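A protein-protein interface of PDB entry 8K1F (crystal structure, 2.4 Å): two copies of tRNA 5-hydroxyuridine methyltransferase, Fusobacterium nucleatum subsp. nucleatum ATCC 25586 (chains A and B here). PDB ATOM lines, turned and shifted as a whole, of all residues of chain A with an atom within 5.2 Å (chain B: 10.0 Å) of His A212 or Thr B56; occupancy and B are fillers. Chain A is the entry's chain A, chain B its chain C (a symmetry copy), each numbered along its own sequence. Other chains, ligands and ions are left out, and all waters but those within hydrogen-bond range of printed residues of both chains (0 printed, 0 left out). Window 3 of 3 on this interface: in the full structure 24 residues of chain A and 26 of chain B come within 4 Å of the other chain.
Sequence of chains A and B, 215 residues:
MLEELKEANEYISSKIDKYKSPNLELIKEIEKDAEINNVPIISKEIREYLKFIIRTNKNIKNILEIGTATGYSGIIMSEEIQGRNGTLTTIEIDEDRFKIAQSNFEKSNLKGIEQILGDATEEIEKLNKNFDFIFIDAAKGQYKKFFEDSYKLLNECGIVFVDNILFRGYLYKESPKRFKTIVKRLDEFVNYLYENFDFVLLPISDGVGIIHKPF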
ATOM      1  N   TYR A 151     -10.298 -16.331 -19.931  1.00  0.00           N
ATOM      2  CA  TYR A 151      -9.224 -16.203 -20.914  1.00  0.00           C
ATOM      3  C   TYR A 151      -9.770 -16.097 -22.327  1.00  0.00           C
ATOM      4  O   TYR A 151      -9.172 -15.434 -23.180  1.00  0.00           O
ATOM      5  CB  TYR A 151      -8.267 -17.385 -20.804  1.00  0.00           C
ATOM      6  CG  TYR A 151      -7.032 -17.281 -21.686  1.00  0.00           C
ATOM      7  CD1 TYR A 151      -5.879 -16.651 -21.230  1.00  0.00           C
ATOM      8  CD2 TYR A 151      -7.021 -17.826 -22.974  1.00  0.00           C
ATOM      9  CE1 TYR A 151      -4.749 -16.555 -22.031  1.00  0.00           C
ATOM     10  CE2 TYR A 151      -5.908 -17.747 -23.783  1.00  0.00           C
ATOM     11  CZ  TYR A 151      -4.763 -17.117 -23.310  1.00  0.00           C
ATOM     12  OH  TYR A 151      -3.644 -17.037 -24.121  1.00  0.00           O
ATOM     13  N   CYS A 157      -2.812  -9.429 -26.701  1.00  0.00           N
ATOM     14  CA  CYS A 157      -1.894  -8.635 -25.874  1.00  0.00           C
ATOM     15  C   CYS A 157      -2.461  -8.362 -24.465  1.00  0.00           C
ATOM     16  O   CYS A 157      -2.070  -7.398 -23.796  1.00  0.00           O
ATOM     17  CB  CYS A 157      -1.522  -7.326 -26.587  1.00  0.00           C
ATOM     18  SG  CYS A 157      -0.735  -7.603 -28.166  1.00  0.00           S
ATOM     19  N   GLY A 158      -3.383  -9.219 -23.988  1.00  0.00           N
ATOM     20  CA  GLY A 158      -3.992  -9.056 -22.686  1.00  0.00           C
ATOM     21  C   GLY A 158      -3.353  -9.913 -21.590  1.00  0.00           C
ATOM     22  O   GLY A 158      -2.711 -10.929 -21.845  1.00  0.00           O
ATOM     23  N   ILE A 159      -3.568  -9.495 -20.347  1.00  0.00           N
ATOM     24  CA  ILE A 159      -2.905 -10.062 -19.179  1.00  0.00           C
ATOM     25  C   ILE A 159      -3.970 -10.623 -18.250  1.00  0.00           C
ATOM     26  O   ILE A 159      -4.952  -9.939 -17.936  1.00  0.00           O
ATOM     27  CB  ILE A 159      -2.064  -8.996 -18.445  1.00  0.00           C
ATOM     28  CG1 ILE A 159      -0.785  -8.651 -19.220  1.00  0.00           C
ATOM     29  CG2 ILE A 159      -1.768  -9.389 -17.004  1.00  0.00           C
ATOM     30  CD1 ILE A 159      -0.069  -9.855 -19.791  1.00  0.00           C
ATOM     31  N   ASP A 198       1.996 -18.551 -22.372  1.00  0.00           N
ATOM     32  CA  ASP A 198       3.040 -17.578 -22.075  1.00  0.00           C
ATOM     33  C   ASP A 198       2.866 -17.131 -20.629  1.00  0.00           C
ATOM     34  O   ASP A 198       1.945 -16.376 -20.321  1.00  0.00           O
ATOM     35  CB  ASP A 198       2.905 -16.398 -23.026  1.00  0.00           C
ATOM     36  CG  ASP A 198       4.234 -15.887 -23.543  1.00  0.00           C
ATOM     37  OD1 ASP A 198       5.213 -15.777 -22.767  1.00  0.00           O
ATOM     38  OD2 ASP A 198       4.276 -15.575 -24.759  1.00  0.00           O
ATOM     39  N   PHE A 199       3.751 -17.576 -19.749  1.00  0.00           N
ATOM     40  CA  PHE A 199       3.523 -17.532 -18.309  1.00  0.00           C
ATOM     41  C   PHE A 199       4.859 -17.299 -17.608  1.00  0.00           C
ATOM     42  O   PHE A 199       5.874 -17.879 -18.011  1.00  0.00           O
ATOM     43  CB  PHE A 199       2.857 -18.848 -17.871  1.00  0.00           C
ATOM     44  CG  PHE A 199       2.624 -18.968 -16.395  1.00  0.00           C
ATOM     45  CD1 PHE A 199       1.818 -18.058 -15.725  1.00  0.00           C
ATOM     46  CD2 PHE A 199       3.185 -20.019 -15.677  1.00  0.00           C
ATOM     47  CE1 PHE A 199       1.602 -18.183 -14.342  1.00  0.00           C
ATOM     48  CE2 PHE A 199       2.973 -20.144 -14.320  1.00  0.00           C
ATOM     49  CZ  PHE A 199       2.188 -19.219 -13.650  1.00  0.00           C
ATOM     50  N   ILE A 210       1.680 -14.392 -14.066  1.00  0.00           N
ATOM     51  CA  ILE A 210       1.276 -13.521 -15.164  1.00  0.00           C
ATOM     52  C   ILE A 210       1.161 -14.358 -16.433  1.00  0.00           C
ATOM     53  O   ILE A 210       2.134 -14.995 -16.852  1.00  0.00           O
ATOM     54  CB  ILE A 210       2.261 -12.364 -15.381  1.00  0.00           C
ATOM     55  CG1 ILE A 210       2.527 -11.607 -14.095  1.00  0.00           C
ATOM     56  CG2 ILE A 210       1.691 -11.394 -16.416  1.00  0.00           C
ATOM     57  CD1 ILE A 210       1.384 -10.727 -13.723  1.00  0.00           C
ATOM     58  N   ILE A 211      -0.005 -14.324 -17.071  1.00  0.00           N
ATOM     59  CA  ILE A 211      -0.199 -14.941 -18.375  1.00  0.00           C
ATOM     60  C   ILE A 211      -0.483 -13.856 -19.392  1.00  0.00           C
ATOM     61  O   ILE A 211      -1.347 -13.002 -19.164  1.00  0.00           O
ATOM     62  CB  ILE A 211      -1.341 -15.959 -18.373  1.00  0.00           C
ATOM     63  CG1 ILE A 211      -1.057 -17.096 -17.398  1.00  0.00           C
ATOM     64  CG2 ILE A 211      -1.583 -16.453 -19.816  1.00  0.00           C
ATOM     65  CD1 ILE A 211      -1.472 -16.803 -15.963  1.00  0.00           C
ATOM     66  N   HIS A 212       0.217 -13.917 -20.522  1.00  0.00           N
ATOM     67  CA  HIS A 212       0.071 -12.984 -21.633  1.00  0.00           C
ATOM     68  C   HIS A 212      -0.545 -13.697 -22.825  1.00  0.00           C
ATOM     69  O   HIS A 212      -0.214 -14.851 -23.111  1.00  0.00           O
ATOM     70  CB  HIS A 212       1.420 -12.397 -22.030  1.00  0.00           C
ATOM     71  CG  HIS A 212       1.338 -11.428 -23.162  1.00  0.00           C
ATOM     72  ND1 HIS A 212       1.540 -11.799 -24.473  1.00  0.00           N
ATOM     73  CD2 HIS A 212       1.080 -10.097 -23.183  1.00  0.00           C
ATOM     74  CE1 HIS A 212       1.403 -10.741 -25.253  1.00  0.00           C
ATOM     75  NE2 HIS A 212       1.121  -9.695 -24.497  1.00  0.00           N
ATOM     76  N   LYS A 213      -1.467 -13.029 -23.502  1.00  0.00           N
ATOM     77  CA  LYS A 213      -2.161 -13.644 -24.624  1.00  0.00           C
ATOM     78  C   LYS A 213      -1.621 -13.040 -25.905  1.00  0.00           C
ATOM     79  O   LYS A 213      -1.764 -11.826 -26.109  1.00  0.00           O
ATOM     80  CB  LYS A 213      -3.677 -13.441 -24.525  1.00  0.00           C
ATOM     81  CG  LYS A 213      -4.507 -14.356 -25.435  1.00  0.00           C
ATOM     82  CD  LYS A 213      -5.981 -14.267 -25.094  1.00  0.00           C
ATOM     83  CE  LYS A 213      -6.848 -15.052 -26.057  1.00  0.00           C
ATOM     84  NZ  LYS A 213      -8.301 -14.803 -25.827  1.00  0.00           N
ATOM     85  N   PRO A 214      -0.988 -13.835 -26.781  1.00  0.00           N
ATOM     86  CA  PRO A 214      -0.243 -13.420 -27.976  1.00  0.00           C
ATOM     87  C   PRO A 214      -1.023 -12.541 -28.946  1.00  0.00           C
ATOM     88  O   PRO A 214      -2.251 -12.600 -28.949  1.00  0.00           O
ATOM     89  CB  PRO A 214       0.113 -14.754 -28.640  1.00  0.00           C
ATOM     90  CG  PRO A 214      -0.699 -15.800 -27.942  1.00  0.00           C
ATOM     91  CD  PRO A 214      -0.934 -15.292 -26.580  1.00  0.00           C
ATOM     92  N   LYS B  20      10.898 -24.132 -19.373  1.00  0.00           N
ATOM     93  CA  LYS B  20      11.458 -22.962 -20.034  1.00  0.00           C
ATOM     94  C   LYS B  20      12.930 -23.164 -20.382  1.00  0.00           C
ATOM     95  O   LYS B  20      13.724 -22.229 -20.350  1.00  0.00           O
ATOM     96  CB  LYS B  20      11.260 -21.712 -19.180  1.00  0.00           C
ATOM     97  CG  LYS B  20       9.802 -21.436 -18.829  1.00  0.00           C
ATOM     98  CD  LYS B  20       8.935 -21.316 -20.062  1.00  0.00           C
ATOM     99  CE  LYS B  20       8.734 -19.866 -20.462  1.00  0.00           C
ATOM    100  NZ  LYS B  20       8.822 -19.625 -21.950  1.00  0.00           N
ATOM    101  N   GLU B  48      14.172 -15.629 -17.261  1.00  0.00           N
ATOM    102  CA  GLU B  48      12.827 -15.825 -17.792  1.00  0.00           C
ATOM    103  C   GLU B  48      11.982 -14.563 -17.695  1.00  0.00           C
ATOM    104  O   GLU B  48      11.108 -14.333 -18.541  1.00  0.00           O
ATOM    105  CB  GLU B  48      12.146 -16.976 -17.061  1.00  0.00           C
ATOM    106  CG  GLU B  48      12.701 -18.331 -17.419  1.00  0.00           C
ATOM    107  CD  GLU B  48      12.875 -18.525 -18.935  1.00  0.00           C
ATOM    108  OE1 GLU B  48      13.964 -19.005 -19.359  1.00  0.00           O
ATOM    109  OE2 GLU B  48      11.926 -18.209 -19.707  1.00  0.00           O
ATOM    110  N   TYR B  49      12.214 -13.740 -16.675  1.00  0.00           N
ATOM    111  CA  TYR B  49      11.451 -12.508 -16.528  1.00  0.00           C
ATOM    112  C   TYR B  49      11.840 -11.512 -17.610  1.00  0.00           C
ATOM    113  O   TYR B  49      10.992 -11.032 -18.373  1.00  0.00           O
ATOM    114  CB  TYR B  49      11.679 -11.934 -15.130  1.00  0.00           C
ATOM    115  CG  TYR B  49      10.835 -10.725 -14.788  1.00  0.00           C
ATOM    116  CD1 TYR B  49       9.448 -10.749 -14.922  1.00  0.00           C
ATOM    117  CD2 TYR B  49      11.427  -9.558 -14.314  1.00  0.00           C
ATOM    118  CE1 TYR B  49       8.676  -9.634 -14.599  1.00  0.00           C
ATOM    119  CE2 TYR B  49      10.661  -8.441 -13.978  1.00  0.00           C
ATOM    120  CZ  TYR B  49       9.291  -8.488 -14.123  1.00  0.00           C
ATOM    121  OH  TYR B  49       8.539  -7.375 -13.804  1.00  0.00           O
ATOM    122  N   LEU B  50      13.133 -11.194 -17.684  1.00  0.00           N
ATOM    123  CA  LEU B  50      13.722 -10.497 -18.820  1.00  0.00           C
ATOM    124  C   LEU B  50      13.168 -11.005 -20.155  1.00  0.00           C
ATOM    125  O   LEU B  50      12.602 -10.240 -20.949  1.00  0.00           O
ATOM    126  CB  LEU B  50      15.241 -10.688 -18.735  1.00  0.00           C
ATOM    127  CG  LEU B  50      16.298  -9.627 -19.028  1.00  0.00           C
ATOM    128  CD1 LEU B  50      15.904  -8.194 -18.629  1.00  0.00           C
ATOM    129  CD2 LEU B  50      17.591 -10.075 -18.358  1.00  0.00           C
ATOM    130  N   LYS B  51      13.319 -12.310 -20.411  1.00  0.00           N
ATOM    131  CA  LYS B  51      12.778 -12.898 -21.633  1.00  0.00           C
ATOM    132  C   LYS B  51      11.294 -12.584 -21.794  1.00  0.00           C
ATOM    133  O   LYS B  51      10.834 -12.260 -22.893  1.00  0.00           O
ATOM    134  CB  LYS B  51      12.989 -14.415 -21.622  1.00  0.00           C
ATOM    135  CG  LYS B  51      14.321 -14.891 -22.169  1.00  0.00           C
ATOM    136  CD  LYS B  51      14.275 -16.379 -22.431  1.00  0.00           C
ATOM    137  CE  LYS B  51      15.532 -16.868 -23.103  1.00  0.00           C
ATOM    138  NZ  LYS B  51      16.074 -15.941 -24.134  1.00  0.00           N
ATOM    139  N   PHE B  52      10.533 -12.665 -20.704  1.00  0.00           N
ATOM    140  CA  PHE B  52       9.089 -12.447 -20.759  1.00  0.00           C
ATOM    141  C   PHE B  52       8.751 -10.999 -21.124  1.00  0.00           C
ATOM    142  O   PHE B  52       7.983 -10.757 -22.059  1.00  0.00           O
ATOM    143  CB  PHE B  52       8.471 -12.856 -19.412  1.00  0.00           C
ATOM    144  CG  PHE B  52       6.975 -12.788 -19.358  1.00  0.00           C
ATOM    145  CD1 PHE B  52       6.329 -11.603 -19.025  1.00  0.00           C
ATOM    146  CD2 PHE B  52       6.210 -13.912 -19.604  1.00  0.00           C
ATOM    147  CE1 PHE B  52       4.944 -11.535 -18.960  1.00  0.00           C
ATOM    148  CE2 PHE B  52       4.829 -13.853 -19.542  1.00  0.00           C
ATOM    149  CZ  PHE B  52       4.193 -12.655 -19.212  1.00  0.00           C
ATOM    150  N   ILE B  53       9.308 -10.020 -20.400  1.00  0.00           N
ATOM    151  CA  ILE B  53       9.016  -8.607 -20.683  1.00  0.00           C
ATOM    152  C   ILE B  53       9.273  -8.293 -22.148  1.00  0.00           C
ATOM    153  O   ILE B  53       8.459  -7.647 -22.818  1.00  0.00           O
ATOM    154  CB  ILE B  53       9.862  -7.681 -19.790  1.00  0.00           C
ATOM    155  CG1 ILE B  53       9.388  -7.681 -18.346  1.00  0.00           C
ATOM    156  CG2 ILE B  53       9.835  -6.286 -20.321  1.00  0.00           C
ATOM    157  CD1 ILE B  53      10.528  -7.430 -17.380  1.00  0.00           C
ATOM    158  N   ILE B  54      10.424  -8.723 -22.665  1.00  0.00           N
ATOM    159  CA  ILE B  54      10.806  -8.354 -24.025  1.00  0.00           C
ATOM    160  C   ILE B  54       9.846  -8.963 -25.038  1.00  0.00           C
ATOM    161  O   ILE B  54       9.444  -8.314 -26.015  1.00  0.00           O
ATOM    162  CB  ILE B  54      12.256  -8.786 -24.289  1.00  0.00           C
ATOM    163  CG1 ILE B  54      13.197  -8.102 -23.308  1.00  0.00           C
ATOM    164  CG2 ILE B  54      12.674  -8.424 -25.680  1.00  0.00           C
ATOM    165  CD1 ILE B  54      14.596  -8.573 -23.465  1.00  0.00           C
ATOM    166  N   ARG B  55       9.449 -10.212 -24.805  1.00  0.00           N
ATOM    167  CA  ARG B  55       8.565 -10.919 -25.724  1.00  0.00           C
ATOM    168  C   ARG B  55       7.177 -10.305 -25.747  1.00  0.00           C
ATOM    169  O   ARG B  55       6.544 -10.236 -26.804  1.00  0.00           O
ATOM    170  CB  ARG B  55       8.493 -12.390 -25.319  1.00  0.00           C
ATOM    171  CG  ARG B  55       7.493 -13.260 -26.068  1.00  0.00           C
ATOM    172  CD  ARG B  55       7.298 -14.555 -25.263  1.00  0.00           C
ATOM    173  NE  ARG B  55       8.549 -14.970 -24.620  1.00  0.00           N
ATOM    174  CZ  ARG B  55       8.651 -15.466 -23.383  1.00  0.00           C
ATOM    175  NH1 ARG B  55       7.574 -15.627 -22.614  1.00  0.00           N
ATOM    176  NH2 ARG B  55       9.839 -15.823 -22.917  1.00  0.00           N
ATOM    177  N   THR B  56       6.676  -9.860 -24.597  1.00  0.00           N
ATOM    178  CA  THR B  56       5.293  -9.415 -24.550  1.00  0.00           C
ATOM    179  C   THR B  56       5.126  -7.947 -24.914  1.00  0.00           C
ATOM    180  O   THR B  56       3.988  -7.460 -24.921  1.00  0.00           O
ATOM    181  CB  THR B  56       4.691  -9.702 -23.171  1.00  0.00           C
ATOM    182  OG1 THR B  56       5.175  -8.757 -22.205  1.00  0.00           O
ATOM    183  CG2 THR B  56       5.071 -11.114 -22.748  1.00  0.00           C
ATOM    184  N   ASN B  57       6.215  -7.237 -25.217  1.00  0.00           N
ATOM    185  CA  ASN B  57       6.161  -5.844 -25.672  1.00  0.00           C
ATOM    186  C   ASN B  57       6.750  -5.811 -27.070  1.00  0.00           C
ATOM    187  O   ASN B  57       7.960  -5.643 -27.236  1.00  0.00           O
ATOM    188  CB  ASN B  57       6.915  -4.926 -24.769  1.00  0.00           C
ATOM    189  CG  ASN B  57       6.325  -4.860 -23.392  1.00  0.00           C
ATOM    190  OD1 ASN B  57       5.659  -3.883 -23.039  1.00  0.00           O
ATOM    191  ND2 ASN B  57       6.570  -5.891 -22.589  1.00  0.00           N
ATOM    192  N   LYS B  58       5.894  -5.955 -28.080  1.00  0.00           N
ATOM    193  CA  LYS B  58       6.379  -5.952 -29.449  1.00  0.00           C
ATOM    194  C   LYS B  58       7.057  -4.643 -29.816  1.00  0.00           C
ATOM    195  O   LYS B  58       7.730  -4.588 -30.844  1.00  0.00           O
ATOM    196  CB  LYS B  58       5.223  -6.237 -30.408  1.00  0.00           C
ATOM    197  N   ASN B  59       6.903  -3.600 -29.006  1.00  0.00           N
ATOM    198  CA  ASN B  59       7.541  -2.313 -29.244  1.00  0.00           C
ATOM    199  C   ASN B  59       8.982  -2.264 -28.729  1.00  0.00           C
ATOM    200  O   ASN B  59       9.668  -1.252 -28.935  1.00  0.00           O
ATOM    201  CB  ASN B  59       6.708  -1.195 -28.602  1.00  0.00           C
ATOM    202  N   ILE B  60       9.461  -3.322 -28.074  1.00  0.00           N
ATOM    203  CA  ILE B  60      10.852  -3.388 -27.637  1.00  0.00           C
ATOM    204  C   ILE B  60      11.672  -3.840 -28.840  1.00  0.00           C
ATOM    205  O   ILE B  60      11.689  -5.026 -29.178  1.00  0.00           O
ATOM    206  CB  ILE B  60      11.043  -4.325 -26.444  1.00  0.00           C
ATOM    207  CG1 ILE B  60      10.467  -3.701 -25.170  1.00  0.00           C
ATOM    208  CG2 ILE B  60      12.522  -4.663 -26.288  1.00  0.00           C
ATOM    209  CD1 ILE B  60      10.591  -4.599 -23.942  1.00  0.00           C
ATOM    210  N   LYS B  61      12.360  -2.896 -29.487  1.00  0.00           N
ATOM    211  CA  LYS B  61      13.115  -3.149 -30.708  1.00  0.00           C
ATOM    212  C   LYS B  61      14.619  -2.986 -30.549  1.00  0.00           C
ATOM    213  O   LYS B  61      15.384  -3.806 -31.069  1.00  0.00           O
ATOM    214  CB  LYS B  61      12.611  -2.215 -31.831  1.00  0.00           C
ATOM    215  N   GLU B  80      15.233 -12.918 -27.904  1.00  0.00           N
ATOM    216  CA  GLU B  80      13.824 -12.552 -27.960  1.00  0.00           C
ATOM    217  C   GLU B  80      13.523 -11.480 -29.001  1.00  0.00           C
ATOM    218  O   GLU B  80      12.375 -11.027 -29.068  1.00  0.00           O
ATOM    219  CB  GLU B  80      13.332 -12.065 -26.586  1.00  0.00           C
ATOM    220  CG  GLU B  80      13.587 -13.027 -25.434  1.00  0.00           C
ATOM    221  CD  GLU B  80      12.978 -14.388 -25.698  1.00  0.00           C
ATOM    222  OE1 GLU B  80      11.789 -14.438 -26.068  1.00  0.00           O
ATOM    223  OE2 GLU B  80      13.678 -15.408 -25.537  1.00  0.00           O
ATOM    224  N   ILE B  81      14.489 -11.042 -29.814  1.00  0.00           N
ATOM    225  CA  ILE B  81      14.155  -9.966 -30.749  1.00  0.00           C
ATOM    226  C   ILE B  81      14.563 -10.295 -32.180  1.00  0.00           C
ATOM    227  O   ILE B  81      14.460  -9.443 -33.071  1.00  0.00           O
ATOM    228  CB  ILE B  81      14.767  -8.612 -30.315  1.00  0.00           C
ATOM    229  CG1 ILE B  81      16.287  -8.627 -30.427  1.00  0.00           C
ATOM    230  CG2 ILE B  81      14.314  -8.223 -28.929  1.00  0.00           C
ATOM    231  CD1 ILE B  81      16.898  -7.348 -29.957  1.00  0.00           C
ATOM    232  N   ARG B  84      11.857  -9.600 -34.699  1.00  0.00           N
ATOM    233  CA  ARG B  84      11.549  -8.199 -34.977  1.00  0.00           C
ATOM    234  C   ARG B  84      12.652  -7.482 -35.731  1.00  0.00           C
ATOM    235  O   ARG B  84      12.527  -6.277 -35.964  1.00  0.00           O
ATOM    236  CB  ARG B  84      11.288  -7.433 -33.673  1.00  0.00           C
ATOM    237  CG  ARG B  84      10.679  -8.278 -32.593  1.00  0.00           C
ATOM    238  CD  ARG B  84      10.589  -7.573 -31.255  1.00  0.00           C
ATOM    239  NE  ARG B  84       9.556  -8.223 -30.446  1.00  0.00           N
ATOM    240  CZ  ARG B  84       9.477  -8.195 -29.119  1.00  0.00           C
ATOM    241  NH1 ARG B  84      10.384  -7.546 -28.390  1.00  0.00           N
ATOM    242  NH2 ARG B  84       8.475  -8.827 -28.522  1.00  0.00           N
ATOM    243  N   PHE B 133      14.634  -0.075 -24.245  1.00  0.00           N
ATOM    244  CA  PHE B 133      14.894  -0.964 -23.120  1.00  0.00           C
ATOM    245  C   PHE B 133      16.379  -0.916 -22.778  1.00  0.00           C
ATOM    246  O   PHE B 133      17.239  -1.089 -23.647  1.00  0.00           O
ATOM    247  CB  PHE B 133      14.446  -2.387 -23.453  1.00  0.00           C
ATOM    248  CG  PHE B 133      14.479  -3.341 -22.282  1.00  0.00           C
ATOM    249  CD1 PHE B 133      15.616  -4.023 -21.966  1.00  0.00           C
ATOM    250  CD2 PHE B 133      13.367  -3.585 -21.530  1.00  0.00           C
ATOM    251  CE1 PHE B 133      15.634  -4.896 -20.910  1.00  0.00           C
ATOM    252  CE2 PHE B 133      13.403  -4.469 -20.475  1.00  0.00           C
ATOM    253  CZ  PHE B 133      14.529  -5.130 -20.180  1.00  0.00           C
ATOM    254  N   ILE B 159      11.496   1.053 -21.216  1.00  0.00           N
ATOM    255  CA  ILE B 159      11.667   0.420 -19.916  1.00  0.00           C
ATOM    256  C   ILE B 159      13.147   0.427 -19.556  1.00  0.00           C
ATOM    257  O   ILE B 159      13.990   0.072 -20.388  1.00  0.00           O
ATOM    258  CB  ILE B 159      11.128  -1.029 -19.934  1.00  0.00           C
ATOM    259  CG1 ILE B 159       9.604  -1.061 -19.878  1.00  0.00           C
ATOM    260  CG2 ILE B 159      11.688  -1.826 -18.769  1.00  0.00           C
ATOM    261  CD1 ILE B 159       9.037  -0.491 -18.599  1.00  0.00           C
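Position printed for both chains: 159.
The guanidinium group (NH2) of Arg B84 sits at hydrogen-bond distance from the backbone carbonyl oxygen (O) of Arg B55, at 2.9 Å. The backbone NH (N) of His A212 is in hydrogen-bond range of the backbone carbonyl oxygen (O) of Asp A198 (3.0 Å). The side-chain hydroxyl (OG1) of Thr B56 lies within hydrogen-bond range of the side-chain amide nitrogen (ND2) of Asn B57, 3.2 Å away. The guanidinium group of Arg B55 lies within salt-bridge range of the side-chain carboxylate of Glu B80 (3.6 Å). OG1 of Thr B56 lies close to O of Phe B52 (3.5 Å).
Among the printed residues, merely in contact across the chains: Asp A198 with Phe B52 (3.8 Å), Phe A199 with Phe B52 (3.9 Å), Ile A210 with Phe B52 (3.9 Å), His A212 with Phe B52 (3.96 Å) and His A212 with Thr B56 (3.6 Å).
Of chain B, only Phe B52 and Thr B56 come within 4 Å of His A212. Thr B56 touches just one residue of chain A: His A212. No residue of chain B comes within 4 Å of Cys A157. No residue of chain B comes within 4 Å of Gly A158. Of chain B, only Phe B52 and Arg B55 come within 4 Å of Asp A198. No residue of chain B comes within 4 Å of Ile A211. No residue of chain B comes within 4 Å of Pro A214. Of the printed residues of chain A, Arg B55 touches Asp A198 (2.4 Å). Of the printed residues of chain B, Ile A210 touches Phe B52. Of the printed residues of chain A, Phe B52 touches Asp A198, Phe A199, Ile A210 and His A212. The nearest residue of chain A that does not touch Thr B56 is Asp A198 (4.7 Å).
Printed residues of chain A that touch a printed residue of chain B: Asp A198, Phe A199, Ile A210 and His A212. Hydrophobic or aromatic side chains of chain A that line the printed part of chain B: Ile A210 and His A212. Printed residues of chain B that touch a printed residue of chain A: Phe B52, Arg B55 and Thr B56. Hydrophobic or aromatic side chains of chain B that line the printed part of chain A: Phe B52. Along chain B the printed residues that touch a printed residue of chain A span positions 52 to 56. Among the printed residues, 6 pairs touch across the chains.
The side-chain carboxylate (OD1) of Asp A198 is in salt-bridge range of the guanidinium group (NE) of Arg B55, at 3.9 Å.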
